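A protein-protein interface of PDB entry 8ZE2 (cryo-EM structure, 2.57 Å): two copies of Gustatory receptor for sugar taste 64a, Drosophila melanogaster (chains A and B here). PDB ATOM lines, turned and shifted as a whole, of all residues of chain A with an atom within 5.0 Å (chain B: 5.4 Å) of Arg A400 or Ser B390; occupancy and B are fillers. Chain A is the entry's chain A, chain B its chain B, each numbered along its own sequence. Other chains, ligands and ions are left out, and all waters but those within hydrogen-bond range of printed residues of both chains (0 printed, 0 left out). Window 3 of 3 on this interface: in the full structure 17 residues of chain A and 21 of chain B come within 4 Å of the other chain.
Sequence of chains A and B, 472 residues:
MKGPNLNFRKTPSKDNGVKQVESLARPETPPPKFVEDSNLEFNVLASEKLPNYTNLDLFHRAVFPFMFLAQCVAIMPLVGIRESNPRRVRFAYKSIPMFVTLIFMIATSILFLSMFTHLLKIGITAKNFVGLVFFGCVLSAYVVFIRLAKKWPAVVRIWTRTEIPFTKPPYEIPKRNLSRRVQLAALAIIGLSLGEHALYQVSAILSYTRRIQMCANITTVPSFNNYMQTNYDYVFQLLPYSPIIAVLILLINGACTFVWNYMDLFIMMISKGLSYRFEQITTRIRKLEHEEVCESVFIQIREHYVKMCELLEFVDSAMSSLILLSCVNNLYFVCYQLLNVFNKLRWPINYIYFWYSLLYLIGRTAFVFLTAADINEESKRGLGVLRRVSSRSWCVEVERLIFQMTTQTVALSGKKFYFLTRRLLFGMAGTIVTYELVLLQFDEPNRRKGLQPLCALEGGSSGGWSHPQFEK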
ATOM      1  N   ARG A 302      29.477  -4.603   3.040  1.00  0.00           N
ATOM      2  CA  ARG A 302      28.495  -4.318   2.000  1.00  0.00           C
ATOM      3  C   ARG A 302      28.832  -5.052   0.710  1.00  0.00           C
ATOM      4  O   ARG A 302      27.937  -5.549   0.020  1.00  0.00           O
ATOM      5  CB  ARG A 302      28.415  -2.813   1.746  1.00  0.00           C
ATOM      6  CG  ARG A 302      27.214  -2.394   0.914  1.00  0.00           C
ATOM      7  CD  ARG A 302      27.350  -0.973   0.397  1.00  0.00           C
ATOM      8  NE  ARG A 302      28.446  -0.845  -0.556  1.00  0.00           N
ATOM      9  CZ  ARG A 302      28.387  -1.238  -1.821  1.00  0.00           C
ATOM     10  NH1 ARG A 302      27.293  -1.781  -2.327  1.00  0.00           N
ATOM     11  NH2 ARG A 302      29.456  -1.082  -2.599  1.00  0.00           N
ATOM     12  N   VAL A 396      27.745   6.906   5.130  1.00  0.00           N
ATOM     13  CA  VAL A 396      26.954   6.673   3.920  1.00  0.00           C
ATOM     14  C   VAL A 396      26.790   5.188   3.605  1.00  0.00           C
ATOM     15  O   VAL A 396      25.688   4.736   3.275  1.00  0.00           O
ATOM     16  CB  VAL A 396      27.564   7.414   2.714  1.00  0.00           C
ATOM     17  CG1 VAL A 396      26.669   7.271   1.495  1.00  0.00           C
ATOM     18  CG2 VAL A 396      27.782   8.883   3.049  1.00  0.00           C
ATOM     19  N   GLU A 397      27.884   4.423   3.680  1.00  0.00           N
ATOM     20  CA  GLU A 397      27.840   3.012   3.302  1.00  0.00           C
ATOM     21  C   GLU A 397      26.843   2.235   4.153  1.00  0.00           C
ATOM     22  O   GLU A 397      26.119   1.373   3.642  1.00  0.00           O
ATOM     23  CB  GLU A 397      29.233   2.396   3.417  1.00  0.00           C
ATOM     24  CG  GLU A 397      30.316   3.197   2.724  1.00  0.00           C
ATOM     25  CD  GLU A 397      30.182   3.173   1.217  1.00  0.00           C
ATOM     26  OE1 GLU A 397      30.027   2.070   0.649  1.00  0.00           O
ATOM     27  OE2 GLU A 397      30.232   4.256   0.597  1.00  0.00           O
ATOM     28  N   VAL A 398      26.798   2.521   5.456  1.00  0.00           N
ATOM     29  CA  VAL A 398      25.813   1.874   6.318  1.00  0.00           C
ATOM     30  C   VAL A 398      24.403   2.249   5.887  1.00  0.00           C
ATOM     31  O   VAL A 398      23.480   1.430   5.962  1.00  0.00           O
ATOM     32  CB  VAL A 398      26.066   2.231   7.793  1.00  0.00           C
ATOM     33  CG1 VAL A 398      25.341   1.253   8.703  1.00  0.00           C
ATOM     34  CG2 VAL A 398      27.546   2.219   8.083  1.00  0.00           C
ATOM     35  N   GLU A 399      24.210   3.491   5.437  1.00  0.00           N
ATOM     36  CA  GLU A 399      22.901   3.896   4.935  1.00  0.00           C
ATOM     37  C   GLU A 399      22.507   3.082   3.710  1.00  0.00           C
ATOM     38  O   GLU A 399      21.367   2.615   3.605  1.00  0.00           O
ATOM     39  CB  GLU A 399      22.904   5.392   4.612  1.00  0.00           C
ATOM     40  CG  GLU A 399      21.746   5.931   3.742  1.00  0.00           C
ATOM     41  CD  GLU A 399      20.329   5.577   4.210  1.00  0.00           C
ATOM     42  OE1 GLU A 399      19.380   6.164   3.649  1.00  0.00           O
ATOM     43  OE2 GLU A 399      20.136   4.758   5.133  1.00  0.00           O
ATOM     44  N   ARG A 400      23.446   2.891   2.779  1.00  0.00           N
ATOM     45  CA  ARG A 400      23.176   2.068   1.603  1.00  0.00           C
ATOM     46  C   ARG A 400      22.845   0.637   2.002  1.00  0.00           C
ATOM     47  O   ARG A 400      21.906   0.034   1.474  1.00  0.00           O
ATOM     48  CB  ARG A 400      24.379   2.090   0.659  1.00  0.00           C
ATOM     49  CG  ARG A 400      24.703   3.449   0.064  1.00  0.00           C
ATOM     50  CD  ARG A 400      25.799   3.323  -0.981  1.00  0.00           C
ATOM     51  NE  ARG A 400      25.551   2.211  -1.890  1.00  0.00           N
ATOM     52  CZ  ARG A 400      26.341   1.874  -2.900  1.00  0.00           C
ATOM     53  NH1 ARG A 400      27.458   2.536  -3.155  1.00  0.00           N
ATOM     54  NH2 ARG A 400      26.001   0.847  -3.674  1.00  0.00           N
ATOM     55  N   LEU A 401      23.614   0.077   2.938  1.00  0.00           N
ATOM     56  CA  LEU A 401      23.409  -1.309   3.349  1.00  0.00           C
ATOM     57  C   LEU A 401      22.063  -1.486   4.049  1.00  0.00           C
ATOM     58  O   LEU A 401      21.363  -2.489   3.838  1.00  0.00           O
ATOM     59  CB  LEU A 401      24.564  -1.738   4.254  1.00  0.00           C
ATOM     60  CG  LEU A 401      24.910  -3.222   4.360  1.00  0.00           C
ATOM     61  CD1 LEU A 401      24.788  -3.914   3.012  1.00  0.00           C
ATOM     62  CD2 LEU A 401      26.299  -3.422   4.952  1.00  0.00           C
ATOM     63  N   ILE A 402      21.688  -0.519   4.891  1.00  0.00           N
ATOM     64  CA  ILE A 402      20.401  -0.566   5.575  1.00  0.00           C
ATOM     65  C   ILE A 402      19.263  -0.455   4.572  1.00  0.00           C
ATOM     66  O   ILE A 402      18.292  -1.214   4.630  1.00  0.00           O
ATOM     67  CB  ILE A 402      20.325   0.541   6.642  1.00  0.00           C
ATOM     68  CG1 ILE A 402      21.204   0.183   7.845  1.00  0.00           C
ATOM     69  CG2 ILE A 402      18.884   0.788   7.071  1.00  0.00           C
ATOM     70  CD1 ILE A 402      20.939   1.028   9.070  1.00  0.00           C
ATOM     71  N   PHE A 403      19.372   0.489   3.631  1.00  0.00           N
ATOM     72  CA  PHE A 403      18.369   0.615   2.579  1.00  0.00           C
ATOM     73  C   PHE A 403      18.253  -0.680   1.783  1.00  0.00           C
ATOM     74  O   PHE A 403      17.147  -1.107   1.425  1.00  0.00           O
ATOM     75  CB  PHE A 403      18.742   1.788   1.668  1.00  0.00           C
ATOM     76  CG  PHE A 403      17.727   2.092   0.602  1.00  0.00           C
ATOM     77  CD1 PHE A 403      16.378   1.865   0.812  1.00  0.00           C
ATOM     78  CD2 PHE A 403      18.131   2.615  -0.615  1.00  0.00           C
ATOM     79  CE1 PHE A 403      15.453   2.154  -0.174  1.00  0.00           C
ATOM     80  CE2 PHE A 403      17.210   2.903  -1.603  1.00  0.00           C
ATOM     81  CZ  PHE A 403      15.869   2.671  -1.382  1.00  0.00           C
ATOM     82  N   GLN A 404      19.389  -1.332   1.530  1.00  0.00           N
ATOM     83  CA  GLN A 404      19.404  -2.572   0.765  1.00  0.00           C
ATOM     84  C   GLN A 404      18.642  -3.673   1.491  1.00  0.00           C
ATOM     85  O   GLN A 404      17.651  -4.202   0.975  1.00  0.00           O
ATOM     86  CB  GLN A 404      20.849  -2.996   0.500  1.00  0.00           C
ATOM     87  CG  GLN A 404      21.044  -3.707  -0.820  1.00  0.00           C
ATOM     88  CD  GLN A 404      22.498  -3.785  -1.235  1.00  0.00           C
ATOM     89  OE1 GLN A 404      23.024  -4.869  -1.481  1.00  0.00           O
ATOM     90  NE2 GLN A 404      23.155  -2.635  -1.317  1.00  0.00           N
ATOM     91  N   GLU B 292      34.140   2.563 -13.897  1.00  0.00           N
ATOM     92  CA  GLU B 292      33.838   3.781 -13.155  1.00  0.00           C
ATOM     93  C   GLU B 292      32.912   4.653 -13.992  1.00  0.00           C
ATOM     94  O   GLU B 292      33.280   5.097 -15.084  1.00  0.00           O
ATOM     95  CB  GLU B 292      35.123   4.523 -12.802  1.00  0.00           C
ATOM     96  CG  GLU B 292      35.957   3.841 -11.728  1.00  0.00           C
ATOM     97  CD  GLU B 292      35.501   4.189 -10.324  1.00  0.00           C
ATOM     98  OE1 GLU B 292      34.955   5.296 -10.130  1.00  0.00           O
ATOM     99  OE2 GLU B 292      35.682   3.353  -9.414  1.00  0.00           O
ATOM    100  N   LEU B 386      22.707  -1.576 -10.333  1.00  0.00           N
ATOM    101  CA  LEU B 386      23.010  -0.324  -9.648  1.00  0.00           C
ATOM    102  C   LEU B 386      23.518  -0.567  -8.234  1.00  0.00           C
ATOM    103  O   LEU B 386      24.345   0.204  -7.734  1.00  0.00           O
ATOM    104  CB  LEU B 386      21.778   0.578  -9.610  1.00  0.00           C
ATOM    105  CG  LEU B 386      21.435   1.311 -10.903  1.00  0.00           C
ATOM    106  CD1 LEU B 386      20.211   2.176 -10.691  1.00  0.00           C
ATOM    107  CD2 LEU B 386      22.616   2.137 -11.369  1.00  0.00           C
ATOM    108  N   ARG B 387      23.035  -1.625  -7.577  1.00  0.00           N
ATOM    109  CA  ARG B 387      23.573  -2.003  -6.276  1.00  0.00           C
ATOM    110  C   ARG B 387      25.025  -2.455  -6.369  1.00  0.00           C
ATOM    111  O   ARG B 387      25.737  -2.431  -5.360  1.00  0.00           O
ATOM    112  CB  ARG B 387      22.715  -3.105  -5.646  1.00  0.00           C
ATOM    113  CG  ARG B 387      21.342  -2.651  -5.161  1.00  0.00           C
ATOM    114  CD  ARG B 387      20.371  -3.820  -5.122  1.00  0.00           C
ATOM    115  NE  ARG B 387      19.131  -3.494  -4.429  1.00  0.00           N
ATOM    116  CZ  ARG B 387      17.973  -4.098  -4.656  1.00  0.00           C
ATOM    117  NH1 ARG B 387      17.866  -5.077  -5.539  1.00  0.00           N
ATOM    118  NH2 ARG B 387      16.895  -3.705  -3.985  1.00  0.00           N
ATOM    119  N   ARG B 388      25.484  -2.848  -7.558  1.00  0.00           N
ATOM    120  CA  ARG B 388      26.874  -3.244  -7.741  1.00  0.00           C
ATOM    121  C   ARG B 388      27.832  -2.064  -7.619  1.00  0.00           C
ATOM    122  O   ARG B 388      29.036  -2.275  -7.433  1.00  0.00           O
ATOM    123  CB  ARG B 388      27.050  -3.873  -9.120  1.00  0.00           C
ATOM    124  CG  ARG B 388      27.860  -5.141  -9.176  1.00  0.00           C
ATOM    125  CD  ARG B 388      27.754  -5.727 -10.581  1.00  0.00           C
ATOM    126  NE  ARG B 388      26.395  -6.048 -11.013  1.00  0.00           N
ATOM    127  CZ  ARG B 388      25.656  -7.034 -10.522  1.00  0.00           C
ATOM    128  NH1 ARG B 388      26.151  -7.899  -9.653  1.00  0.00           N
ATOM    129  NH2 ARG B 388      24.396  -7.170 -10.931  1.00  0.00           N
ATOM    130  N   VAL B 389      27.322  -0.837  -7.727  1.00  0.00           N
ATOM    131  CA  VAL B 389      28.182   0.330  -7.872  1.00  0.00           C
ATOM    132  C   VAL B 389      29.006   0.537  -6.610  1.00  0.00           C
ATOM    133  O   VAL B 389      28.482   0.515  -5.490  1.00  0.00           O
ATOM    134  CB  VAL B 389      27.334   1.566  -8.204  1.00  0.00           C
ATOM    135  CG1 VAL B 389      28.169   2.822  -8.108  1.00  0.00           C
ATOM    136  CG2 VAL B 389      26.727   1.423  -9.592  1.00  0.00           C
ATOM    137  N   SER B 390      30.307   0.742  -6.792  1.00  0.00           N
ATOM    138  CA  SER B 390      31.205   0.967  -5.673  1.00  0.00           C
ATOM    139  C   SER B 390      31.000   2.361  -5.085  1.00  0.00           C
ATOM    140  O   SER B 390      30.249   3.188  -5.611  1.00  0.00           O
ATOM    141  CB  SER B 390      32.659   0.795  -6.112  1.00  0.00           C
ATOM    142  OG  SER B 390      33.171   2.006  -6.644  1.00  0.00           O
ATOM    143  N   SER B 391      31.693   2.615  -3.974  1.00  0.00           N
ATOM    144  CA  SER B 391      31.582   3.896  -3.289  1.00  0.00           C
ATOM    145  C   SER B 391      32.224   5.035  -4.068  1.00  0.00           C
ATOM    146  O   SER B 391      32.006   6.202  -3.724  1.00  0.00           O
ATOM    147  CB  SER B 391      32.219   3.799  -1.902  1.00  0.00           C
ATOM    148  OG  SER B 391      31.779   2.635  -1.226  1.00  0.00           O
ATOM    149  N   ARG B 392      33.007   4.727  -5.104  1.00  0.00           N
ATOM    150  CA  ARG B 392      33.738   5.773  -5.812  1.00  0.00           C
ATOM    151  C   ARG B 392      32.812   6.675  -6.618  1.00  0.00           C
ATOM    152  O   ARG B 392      33.071   7.878  -6.733  1.00  0.00           O
ATOM    153  CB  ARG B 392      34.797   5.153  -6.722  1.00  0.00           C
ATOM    154  CG  ARG B 392      36.118   4.873  -6.023  1.00  0.00           C
ATOM    155  CD  ARG B 392      36.952   6.146  -5.877  1.00  0.00           C
ATOM    156  NE  ARG B 392      37.084   6.907  -7.117  1.00  0.00           N
ATOM    157  CZ  ARG B 392      37.620   6.452  -8.243  1.00  0.00           C
ATOM    158  NH1 ARG B 392      38.148   5.241  -8.323  1.00  0.00           N
ATOM    159  NH2 ARG B 392      37.643   7.240  -9.314  1.00  0.00           N
ATOM    160  N   SER B 393      31.737   6.126  -7.185  1.00  0.00           N
ATOM    161  CA  SER B 393      30.795   6.906  -7.988  1.00  0.00           C
ATOM    162  C   SER B 393      29.378   6.635  -7.489  1.00  0.00           C
ATOM    163  O   SER B 393      28.646   5.839  -8.081  1.00  0.00           O
ATOM    164  CB  SER B 393      30.944   6.570  -9.469  1.00  0.00           C
ATOM    165  OG  SER B 393      30.357   5.314  -9.765  1.00  0.00           O
ATOM    166  N   TRP B 394      28.980   7.332  -6.428  1.00  0.00           N
ATOM    167  CA  TRP B 394      27.620   7.268  -5.910  1.00  0.00           C
ATOM    168  C   TRP B 394      26.816   8.498  -6.300  1.00  0.00           C
ATOM    169  O   TRP B 394      25.718   8.374  -6.851  1.00  0.00           O
ATOM    170  CB  TRP B 394      27.645   7.103  -4.383  1.00  0.00           C
ATOM    171  CG  TRP B 394      26.322   6.732  -3.772  1.00  0.00           C
ATOM    172  CD1 TRP B 394      25.679   7.382  -2.760  1.00  0.00           C
ATOM    173  CD2 TRP B 394      25.493   5.614  -4.120  1.00  0.00           C
ATOM    174  NE1 TRP B 394      24.497   6.746  -2.464  1.00  0.00           N
ATOM    175  CE2 TRP B 394      24.360   5.658  -3.285  1.00  0.00           C
ATOM    176  CE3 TRP B 394      25.596   4.585  -5.061  1.00  0.00           C
ATOM    177  CZ2 TRP B 394      23.339   4.714  -3.360  1.00  0.00           C
ATOM    178  CZ3 TRP B 394      24.581   3.650  -5.135  1.00  0.00           C
ATOM    179  CH2 TRP B 394      23.468   3.720  -4.288  1.00  0.00           C
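No position is printed for both chains.
Of the 7 pairs that touch across the chains among the printed residues, none has its exchanged pair printed and touching as well.
NE of Arg A302 is in salt-bridge range of OE1 of Glu A397 (3.5 Å).
OG of Ser B390 lies close to N of Arg B392, at 3.1 Å.
The backbone carbonyl oxygen (O) of Arg B387 lies within hydrogen-bond range of the guanidinium group (NH1) of Arg A302.
NH2 of Arg A302 lies within hydrogen-bond range of O of Val B389 (3.4 Å).
The side-chain hydroxyl of Ser B391 lies within hydrogen-bond range of the side-chain carboxylate of Glu A397 (2.6 Å).
NH2 of Arg A400 sits at hydrogen-bond distance from O of Val B389, 3.1 Å away.
Among the printed residues, pairs that only touch across the chains: Arg A400 with Trp B394, Arg A400 with Arg B387 and Arg A400 with Ser B390.
Of the 10 printed residues of chain B, 5 touch a printed residue of chain A.
Printed residues of chain B that touch a printed residue of chain A: Arg B387, Val B389, Ser B390, Ser B391 and Trp B394.
Hydrophobic or aromatic side chains of chain B within 4 Å of the printed part of chain A: Trp B394.
Of the 10 printed residues of chain A, 3 touch a printed residue of chain B.
Among the printed residues, 7 pairs touch across the chains.
Printed residues of chain B within 4 Å of Arg A302: Arg B387 and Val B389.
Of the printed residues of chain B, Glu A397 touches Ser B391 (2.6 Å).
Arg A400 touches just these residues of chain B: Arg B387 (3.7 Å), Val B389 (3.1 Å), Ser B390 (3.8 Å) and Trp B394 (3.4 Å).
Ile A402 touches none of the printed residues of chain B.
Glu B292 touches none of the printed residues of chain A.
Printed residues of chain A within 4 Å of Arg B387: Arg A302 (3.5 Å) and Arg A400 (3.7 Å).
Of the printed residues of chain A, Ser B390 touches Arg A400 (3.8 Å).
Of the printed residues of chain A, Ser B391 touches Glu A397.
Of the printed residues of chain A, Trp B394 touches Arg A400 (3.4 Å).
The nearest residue of chain A that does not touch Ser B390 is Arg A302 (4.1 Å).
The nearest printed residue of chain B that does not touch Glu A397 is Ser B390 (5.8 Å).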
